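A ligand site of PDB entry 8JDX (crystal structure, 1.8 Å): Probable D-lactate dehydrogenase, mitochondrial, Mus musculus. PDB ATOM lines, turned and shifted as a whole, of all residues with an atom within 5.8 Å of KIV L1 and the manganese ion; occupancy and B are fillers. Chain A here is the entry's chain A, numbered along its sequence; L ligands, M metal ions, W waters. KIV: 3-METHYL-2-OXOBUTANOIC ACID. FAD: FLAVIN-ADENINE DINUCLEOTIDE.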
ATOM      1  N   VAL A  88     -10.114 -13.898 -16.121  1.00  0.00           N
ATOM      2  CA  VAL A  88     -10.901 -14.444 -15.025  1.00  0.00           C
ATOM      3  C   VAL A  88     -11.273 -15.918 -15.251  1.00  0.00           C
ATOM      4  O   VAL A  88     -12.165 -16.431 -14.589  1.00  0.00           O
ATOM      5  CB  VAL A  88     -12.147 -13.587 -14.739  1.00  0.00           C
ATOM      6  CG1 VAL A  88     -11.734 -12.211 -14.224  1.00  0.00           C
ATOM      7  CG2 VAL A  88     -13.007 -13.442 -16.001  1.00  0.00           C
ATOM      8  N   GLY A 146     -13.179  -3.524 -17.495  1.00  0.00           N
ATOM      9  CA  GLY A 146     -12.940  -2.787 -16.277  1.00  0.00           C
ATOM     10  C   GLY A 146     -11.477  -2.756 -15.871  1.00  0.00           C
ATOM     11  O   GLY A 146     -11.027  -1.809 -15.214  1.00  0.00           O
ATOM     12  N   SER A 160     -15.107  -7.695 -24.520  1.00  0.00           N
ATOM     13  CA  SER A 160     -15.991  -6.570 -24.826  1.00  0.00           C
ATOM     14  C   SER A 160     -15.982  -5.614 -23.633  1.00  0.00           C
ATOM     15  O   SER A 160     -14.979  -5.530 -22.917  1.00  0.00           O
ATOM     16  CB  SER A 160     -17.408  -7.045 -25.193  1.00  0.00           C
ATOM     17  OG  SER A 160     -18.136  -7.515 -24.071  1.00  0.00           O
ATOM     18  N   GLY A 161     -17.075  -4.901 -23.421  1.00  0.00           N
ATOM     19  CA  GLY A 161     -17.126  -3.956 -22.317  1.00  0.00           C
ATOM     20  C   GLY A 161     -18.398  -3.146 -22.377  1.00  0.00           C
ATOM     21  O   GLY A 161     -19.296  -3.450 -23.163  1.00  0.00           O
ATOM     22  N   GLU A 264     -25.840  -0.384 -18.648  1.00  0.00           N
ATOM     23  CA  GLU A 264     -25.259  -1.321 -17.692  1.00  0.00           C
ATOM     24  C   GLU A 264     -26.240  -1.589 -16.566  1.00  0.00           C
ATOM     25  O   GLU A 264     -26.845  -0.652 -16.030  1.00  0.00           O
ATOM     26  CB  GLU A 264     -23.946  -0.771 -17.121  1.00  0.00           C
ATOM     27  CG  GLU A 264     -22.784  -0.800 -18.117  1.00  0.00           C
ATOM     28  CD  GLU A 264     -22.406  -2.211 -18.533  1.00  0.00           C
ATOM     29  OE1 GLU A 264     -22.108  -3.034 -17.642  1.00  0.00           O
ATOM     30  OE2 GLU A 264     -22.391  -2.486 -19.753  1.00  0.00           O
ATOM     31  N   ARG A 334     -18.282   1.559 -11.810  1.00  0.00           N
ATOM     32  CA  ARG A 334     -18.743   0.414 -12.589  1.00  0.00           C
ATOM     33  C   ARG A 334     -17.568  -0.497 -12.958  1.00  0.00           C
ATOM     34  O   ARG A 334     -17.625  -1.710 -12.747  1.00  0.00           O
ATOM     35  CB  ARG A 334     -19.479   0.884 -13.841  1.00  0.00           C
ATOM     36  CG  ARG A 334     -19.690  -0.207 -14.898  1.00  0.00           C
ATOM     37  CD  ARG A 334     -20.582  -1.336 -14.406  1.00  0.00           C
ATOM     38  NE  ARG A 334     -20.628  -2.436 -15.381  1.00  0.00           N
ATOM     39  CZ  ARG A 334     -19.777  -3.457 -15.384  1.00  0.00           C
ATOM     40  NH1 ARG A 334     -18.815  -3.529 -14.472  1.00  0.00           N
ATOM     41  NH2 ARG A 334     -19.880  -4.398 -16.319  1.00  0.00           N
ATOM     42  N   HIS A 335     -16.492   0.091 -13.480  1.00  0.00           N
ATOM     43  CA  HIS A 335     -15.340  -0.699 -13.895  1.00  0.00           C
ATOM     44  C   HIS A 335     -14.703  -1.457 -12.740  1.00  0.00           C
ATOM     45  O   HIS A 335     -14.037  -2.470 -12.975  1.00  0.00           O
ATOM     46  CB  HIS A 335     -14.302   0.202 -14.571  1.00  0.00           C
ATOM     47  CG  HIS A 335     -14.639   0.585 -15.973  1.00  0.00           C
ATOM     48  ND1 HIS A 335     -14.297   1.810 -16.509  1.00  0.00           N
ATOM     49  CD2 HIS A 335     -15.281  -0.079 -16.952  1.00  0.00           C
ATOM     50  CE1 HIS A 335     -14.721   1.879 -17.760  1.00  0.00           C
ATOM     51  NE2 HIS A 335     -15.319   0.739 -18.058  1.00  0.00           N
ATOM     52  N   ALA A 337     -16.495  -2.858 -10.250  1.00  0.00           N
ATOM     53  CA  ALA A 337     -17.531  -3.681  -9.626  1.00  0.00           C
ATOM     54  C   ALA A 337     -16.968  -5.015  -9.146  1.00  0.00           C
ATOM     55  O   ALA A 337     -17.382  -5.527  -8.094  1.00  0.00           O
ATOM     56  CB  ALA A 337     -18.689  -3.909 -10.612  1.00  0.00           C
ATOM     57  N   TRP A 338     -16.054  -5.603  -9.910  1.00  0.00           N
ATOM     58  CA  TRP A 338     -15.413  -6.851  -9.485  1.00  0.00           C
ATOM     59  C   TRP A 338     -14.782  -6.701  -8.109  1.00  0.00           C
ATOM     60  O   TRP A 338     -14.976  -7.551  -7.226  1.00  0.00           O
ATOM     61  CB  TRP A 338     -14.373  -7.269 -10.528  1.00  0.00           C
ATOM     62  CG  TRP A 338     -13.476  -8.440 -10.177  1.00  0.00           C
ATOM     63  CD1 TRP A 338     -12.187  -8.385  -9.740  1.00  0.00           C
ATOM     64  CD2 TRP A 338     -13.791  -9.836 -10.306  1.00  0.00           C
ATOM     65  NE1 TRP A 338     -11.681  -9.653  -9.563  1.00  0.00           N
ATOM     66  CE2 TRP A 338     -12.653 -10.562  -9.898  1.00  0.00           C
ATOM     67  CE3 TRP A 338     -14.934 -10.545 -10.702  1.00  0.00           C
ATOM     68  CZ2 TRP A 338     -12.613 -11.957  -9.893  1.00  0.00           C
ATOM     69  CZ3 TRP A 338     -14.890 -11.928 -10.686  1.00  0.00           C
ATOM     70  CH2 TRP A 338     -13.751 -12.616 -10.293  1.00  0.00           C
ATOM     71  N   SER A 352     -16.809 -15.242 -11.865  1.00  0.00           N
ATOM     72  CA  SER A 352     -17.813 -14.538 -12.645  1.00  0.00           C
ATOM     73  C   SER A 352     -18.406 -15.467 -13.696  1.00  0.00           C
ATOM     74  O   SER A 352     -17.680 -16.170 -14.414  1.00  0.00           O
ATOM     75  CB  SER A 352     -17.217 -13.309 -13.334  1.00  0.00           C
ATOM     76  OG  SER A 352     -18.239 -12.577 -13.979  1.00  0.00           O
ATOM     77  N   ASP A 354     -20.966 -15.376 -17.198  1.00  0.00           N
ATOM     78  CA  ASP A 354     -20.826 -14.486 -18.345  1.00  0.00           C
ATOM     79  C   ASP A 354     -21.726 -14.937 -19.500  1.00  0.00           C
ATOM     80  O   ASP A 354     -21.358 -14.784 -20.669  1.00  0.00           O
ATOM     81  CB  ASP A 354     -19.335 -14.441 -18.755  1.00  0.00           C
ATOM     82  CG  ASP A 354     -19.051 -13.499 -19.924  1.00  0.00           C
ATOM     83  OD1 ASP A 354     -19.654 -12.407 -19.996  1.00  0.00           O
ATOM     84  OD2 ASP A 354     -18.217 -13.864 -20.791  1.00  0.00           O
ATOM     85  N   VAL A 383     -24.210  -7.844 -12.390  1.00  0.00           N
ATOM     86  CA  VAL A 383     -23.806  -6.641 -13.103  1.00  0.00           C
ATOM     87  C   VAL A 383     -23.569  -7.036 -14.558  1.00  0.00           C
ATOM     88  O   VAL A 383     -23.229  -8.183 -14.843  1.00  0.00           O
ATOM     89  CB  VAL A 383     -22.534  -6.020 -12.462  1.00  0.00           C
ATOM     90  CG1 VAL A 383     -21.329  -6.951 -12.643  1.00  0.00           C
ATOM     91  CG2 VAL A 383     -22.235  -4.640 -13.039  1.00  0.00           C
ATOM     92  N   GLY A 384     -23.764  -6.091 -15.472  1.00  0.00           N
ATOM     93  CA  GLY A 384     -23.124  -6.289 -16.754  1.00  0.00           C
ATOM     94  C   GLY A 384     -23.890  -5.707 -17.931  1.00  0.00           C
ATOM     95  O   GLY A 384     -24.782  -4.880 -17.796  1.00  0.00           O
ATOM     96  N   HIS A 385     -23.483  -6.205 -19.104  1.00  0.00           N
ATOM     97  CA  HIS A 385     -23.701  -5.571 -20.393  1.00  0.00           C
ATOM     98  C   HIS A 385     -25.028  -6.056 -20.987  1.00  0.00           C
ATOM     99  O   HIS A 385     -25.076  -6.770 -21.990  1.00  0.00           O
ATOM    100  CB  HIS A 385     -22.528  -5.882 -21.321  1.00  0.00           C
ATOM    101  CG  HIS A 385     -21.193  -5.774 -20.658  1.00  0.00           C
ATOM    102  ND1 HIS A 385     -20.741  -4.608 -20.068  1.00  0.00           N
ATOM    103  CD2 HIS A 385     -20.202  -6.680 -20.484  1.00  0.00           C
ATOM    104  CE1 HIS A 385     -19.543  -4.799 -19.573  1.00  0.00           C
ATOM    105  NE2 HIS A 385     -19.190  -6.051 -19.809  1.00  0.00           N
ATOM    106  N   ASN A 390     -26.210  -9.832 -22.142  1.00  0.00           N
ATOM    107  CA  ASN A 390     -25.081 -10.430 -21.437  1.00  0.00           C
ATOM    108  C   ASN A 390     -25.071  -9.902 -20.000  1.00  0.00           C
ATOM    109  O   ASN A 390     -25.453  -8.763 -19.744  1.00  0.00           O
ATOM    110  CB  ASN A 390     -23.786 -10.054 -22.204  1.00  0.00           C
ATOM    111  CG  ASN A 390     -22.508 -10.450 -21.494  1.00  0.00           C
ATOM    112  OD1 ASN A 390     -21.577  -9.645 -21.420  1.00  0.00           O
ATOM    113  ND2 ASN A 390     -22.414 -11.691 -21.042  1.00  0.00           N
ATOM    114  N   HIS A 392     -23.100 -10.653 -15.777  1.00  0.00           N
ATOM    115  CA  HIS A 392     -22.202 -11.376 -14.883  1.00  0.00           C
ATOM    116  C   HIS A 392     -22.882 -11.593 -13.544  1.00  0.00           C
ATOM    117  O   HIS A 392     -23.440 -10.657 -12.970  1.00  0.00           O
ATOM    118  CB  HIS A 392     -20.903 -10.591 -14.638  1.00  0.00           C
ATOM    119  CG  HIS A 392     -20.222 -10.119 -15.888  1.00  0.00           C
ATOM    120  ND1 HIS A 392     -19.766 -10.989 -16.852  1.00  0.00           N
ATOM    121  CD2 HIS A 392     -19.917  -8.872 -16.318  1.00  0.00           C
ATOM    122  CE1 HIS A 392     -19.208 -10.288 -17.829  1.00  0.00           C
ATOM    123  NE2 HIS A 392     -19.291  -9.006 -17.532  1.00  0.00           N
ATOM    124  N   ILE A 394     -21.391 -12.392 -10.049  1.00  0.00           N
ATOM    125  CA  ILE A 394     -20.107 -12.457  -9.353  1.00  0.00           C
ATOM    126  C   ILE A 394     -20.334 -13.221  -8.056  1.00  0.00           C
ATOM    127  O   ILE A 394     -20.971 -12.716  -7.133  1.00  0.00           O
ATOM    128  CB  ILE A 394     -19.544 -11.054  -9.084  1.00  0.00           C
ATOM    129  CG1 ILE A 394     -19.395 -10.275 -10.395  1.00  0.00           C
ATOM    130  CG2 ILE A 394     -18.196 -11.151  -8.394  1.00  0.00           C
ATOM    131  CD1 ILE A 394     -19.101  -8.805 -10.216  1.00  0.00           C
ATOM    132  N   GLU A 429     -17.832 -12.780 -23.399  1.00  0.00           N
ATOM    133  CA  GLU A 429     -16.589 -12.029 -23.568  1.00  0.00           C
ATOM    134  C   GLU A 429     -15.392 -12.586 -22.791  1.00  0.00           C
ATOM    135  O   GLU A 429     -14.255 -12.426 -23.241  1.00  0.00           O
ATOM    136  CB  GLU A 429     -16.844 -10.571 -23.152  1.00  0.00           C
ATOM    137  CG  GLU A 429     -17.384 -10.430 -21.721  1.00  0.00           C
ATOM    138  CD  GLU A 429     -17.264  -9.028 -21.189  1.00  0.00           C
ATOM    139  OE1 GLU A 429     -17.058  -8.099 -22.002  1.00  0.00           O
ATOM    140  OE2 GLU A 429     -17.371  -8.853 -19.955  1.00  0.00           O
ATOM    141  N   HIS A 430     -15.615 -13.213 -21.631  1.00  0.00           N
ATOM    142  CA  HIS A 430     -14.487 -13.632 -20.795  1.00  0.00           C
ATOM    143  C   HIS A 430     -13.705 -14.798 -21.375  1.00  0.00           C
ATOM    144  O   HIS A 430     -12.499 -14.916 -21.124  1.00  0.00           O
ATOM    145  CB  HIS A 430     -14.971 -14.011 -19.393  1.00  0.00           C
ATOM    146  CG  HIS A 430     -15.401 -12.841 -18.558  1.00  0.00           C
ATOM    147  ND1 HIS A 430     -16.194 -12.975 -17.446  1.00  0.00           N
ATOM    148  CD2 HIS A 430     -15.142 -11.522 -18.687  1.00  0.00           C
ATOM    149  CE1 HIS A 430     -16.410 -11.789 -16.922  1.00  0.00           C
ATOM    150  NE2 HIS A 430     -15.787 -10.887 -17.648  1.00  0.00           N
HETATM  151  O1  KIV L   1     -16.710  -5.496 -14.923  1.00  0.00           O
HETATM  152  C1  KIV L   1     -17.048  -6.392 -15.740  1.00  0.00           C
HETATM  153  O2  KIV L   1     -17.933  -6.155 -16.598  1.00  0.00           O
HETATM  154  C2  KIV L   1     -16.406  -7.772 -15.693  1.00  0.00           C
HETATM  155  C3  KIV L   1     -15.949  -8.301 -14.333  1.00  0.00           C
HETATM  156  C4  KIV L   1     -17.171  -8.646 -13.486  1.00  0.00           C
HETATM  157  C5  KIV L   1     -15.087  -9.558 -14.514  1.00  0.00           C
HETATM  158  O3  KIV L   1     -16.257  -8.408 -16.687  1.00  0.00           O
HETATM  159  PA  FAD L   2      -4.181 -12.599 -19.358  1.00  0.00           P
HETATM  160  O1A FAD L   2      -4.825 -12.997 -18.071  1.00  0.00           O
HETATM  161  O2A FAD L   2      -2.717 -12.196 -19.364  1.00  0.00           O
HETATM  162  O5B FAD L   2      -4.396 -13.762 -20.413  1.00  0.00           O
HETATM  163  C5B FAD L   2      -5.729 -14.163 -20.796  1.00  0.00           C
HETATM  164  C4B FAD L   2      -5.672 -15.321 -21.772  1.00  0.00           C
HETATM  165  O4B FAD L   2      -5.240 -14.834 -23.069  1.00  0.00           O
HETATM  166  C3B FAD L   2      -4.701 -16.439 -21.409  1.00  0.00           C
HETATM  167  O3B FAD L   2      -5.173 -17.692 -21.877  1.00  0.00           O
HETATM  168  C2B FAD L   2      -3.416 -16.007 -22.119  1.00  0.00           C
HETATM  169  O2B FAD L   2      -2.585 -17.125 -22.424  1.00  0.00           O
HETATM  170  C1B FAD L   2      -3.966 -15.357 -23.390  1.00  0.00           C
HETATM  171  N9A FAD L   2      -3.157 -14.262 -23.903  1.00  0.00           N
HETATM  172  C8A FAD L   2      -2.848 -13.090 -23.274  1.00  0.00           C
HETATM  173  N7A FAD L   2      -2.126 -12.260 -23.993  1.00  0.00           N
HETATM  174  C5A FAD L   2      -1.955 -12.948 -25.196  1.00  0.00           C
HETATM  175  C6A FAD L   2      -1.271 -12.622 -26.382  1.00  0.00           C
HETATM  176  N6A FAD L   2      -0.628 -11.468 -26.587  1.00  0.00           N
HETATM  177  N1A FAD L   2      -1.290 -13.528 -27.387  1.00  0.00           N
HETATM  178  C2A FAD L   2      -1.947 -14.677 -27.200  1.00  0.00           C
HETATM  179  N3A FAD L   2      -2.621 -15.098 -26.126  1.00  0.00           N
HETATM  180  C4A FAD L   2      -2.587 -14.179 -25.150  1.00  0.00           C
HETATM  181  N1  FAD L   2     -13.106  -8.896 -19.694  1.00  0.00           N
HETATM  182  C2  FAD L   2     -14.022  -8.482 -20.621  1.00  0.00           C
HETATM  183  O2  FAD L   2     -14.121  -9.024 -21.734  1.00  0.00           O
HETATM  184  N3  FAD L   2     -14.863  -7.426 -20.332  1.00  0.00           N
HETATM  185  C4  FAD L   2     -14.898  -6.714 -19.154  1.00  0.00           C
HETATM  186  O4  FAD L   2     -15.710  -5.806 -19.014  1.00  0.00           O
HETATM  187  C4X FAD L   2     -13.911  -7.153 -18.173  1.00  0.00           C
HETATM  188  N5  FAD L   2     -13.865  -6.519 -17.017  1.00  0.00           N
HETATM  189  C5X FAD L   2     -12.944  -6.942 -16.091  1.00  0.00           C
HETATM  190  C6  FAD L   2     -12.870  -6.279 -14.863  1.00  0.00           C
HETATM  191  C7  FAD L   2     -11.950  -6.662 -13.893  1.00  0.00           C
HETATM  192  C7M FAD L   2     -11.904  -5.933 -12.585  1.00  0.00           C
HETATM  193  C8  FAD L   2     -11.084  -7.742 -14.155  1.00  0.00           C
HETATM  194  C8M FAD L   2     -10.077  -8.177 -13.124  1.00  0.00           C
HETATM  195  C9  FAD L   2     -11.140  -8.396 -15.373  1.00  0.00           C
HETATM  196  C9A FAD L   2     -12.060  -8.013 -16.343  1.00  0.00           C
HETATM  197  N10 FAD L   2     -12.145  -8.656 -17.599  1.00  0.00           N
HETATM  198  C10 FAD L   2     -13.065  -8.254 -18.537  1.00  0.00           C
HETATM  199  C1' FAD L   2     -11.272  -9.807 -17.909  1.00  0.00           C
HETATM  200  C2' FAD L   2      -9.926  -9.425 -18.507  1.00  0.00           C
HETATM  201  O2' FAD L   2      -9.599  -8.075 -18.162  1.00  0.00           O
HETATM  202  C3' FAD L   2      -9.979  -9.593 -20.034  1.00  0.00           C
HETATM  203  O3' FAD L   2     -10.263 -10.958 -20.342  1.00  0.00           O
HETATM  204  C4' FAD L   2      -8.683  -9.201 -20.738  1.00  0.00           C
HETATM  205  O4' FAD L   2      -8.877  -9.269 -22.146  1.00  0.00           O
HETATM  206  C5' FAD L   2      -7.526 -10.101 -20.340  1.00  0.00           C
HETATM  207  O5' FAD L   2      -6.294  -9.542 -20.841  1.00  0.00           O
HETATM  208  P   FAD L   2      -4.914  -9.855 -20.147  1.00  0.00           P
HETATM  209  O1P FAD L   2      -3.757  -9.436 -21.044  1.00  0.00           O
HETATM  210  O2P FAD L   2      -4.914  -9.268 -18.763  1.00  0.00           O
HETATM  211  O3P FAD L   2      -5.033 -11.458 -20.057  1.00  0.00           O
HETATM  212 MN    MN M   1     -17.790  -7.399 -18.435  1.00  0.00          MN
HETATM  213  O   HOH W   1     -15.439  -4.919 -12.543  1.00  0.00           O
HETATM  214  O   HOH W   2     -16.189  -3.032 -16.358  1.00  0.00           O
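The manganese ion is bound by OE2 of Glu 429 (2.1 Å), O2 of KIV L1 (2.2 Å), NE2 of His 392 (2.4 Å), NE2 of His 385 (2.4 Å), O3 of KIV L1 (2.5 Å) and O4 of FAD L2 (2.7 Å).
OE2 of Glu 429 sits close to NE2 of His 430, 3.5 Å away.
The side-chain carboxylate (OE1) of Glu 429 lies within hydrogen-bond range of the backbone NH (N) of Gly 161, 3.5 Å away.
The backbone NH (N) of His 392 lies within hydrogen-bond range of the backbone carbonyl oxygen (O) of Val 383.
A ring nitrogen (ND1) of His 392 lies close to the side-chain carboxylate (OD1) of Asp 354 (3.5 Å).
A ring nitrogen (ND1) of His 385 lies within hydrogen-bond range of the side-chain carboxylate (OE2) of Glu 264 (2.7 Å).
The backbone carbonyl oxygen of His 385 sits at hydrogen-bond distance from the backbone NH of Asn 390 (3.3 Å).
NE of Arg 334 is in salt-bridge range of OE1 of Glu 264 (2.8 Å).
The backbone NH (N) of His 430 is in hydrogen-bond range of the side-chain carboxylate (OD2) of Asp 354 (2.8 Å).
CE3 of Trp 338 touches C5 of KIV L1, at 3.9 Å.
Ile 394 touches KIV L1 (CD1 to C4, 3.8 Å).
Hydrophobic or aromatic side chains within 4 Å of KIV L1: Trp 338, His 385, His 392, Ile 394 and His 430.
Within 4 Å of KIV L1: Arg 334, Trp 338, His 385, His 392, Ile 394, Glu 429 and His 430.
O1 of KIV L1 is in salt-bridge range of NH1 of Arg 334 (2.9 Å).
NE2 of His 430 lies close to O3 of KIV L1, at 2.7 Å.
N of Gly 146 is in hydrogen-bond range of N5 of FAD L2.
The backbone NH (N) of Ser 160 sits at hydrogen-bond distance from an oxygen (O2) of FAD L2 (3.2 Å).
The backbone carbonyl oxygen (O) of Ser 160 lies within hydrogen-bond range of a nitrogen (N3) of FAD L2 (3.2 Å).
Water W1 lies within hydrogen-bond range of O1 of KIV L1 (2.8 Å), N of Trp 338 (2.8 Å), O of His 335 (2.9 Å) and N of Ala 337 (3.3 Å).
Water W2 lies within hydrogen-bond range of O1 of KIV L1, N of Gly 146 and NH1 of Arg 334.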
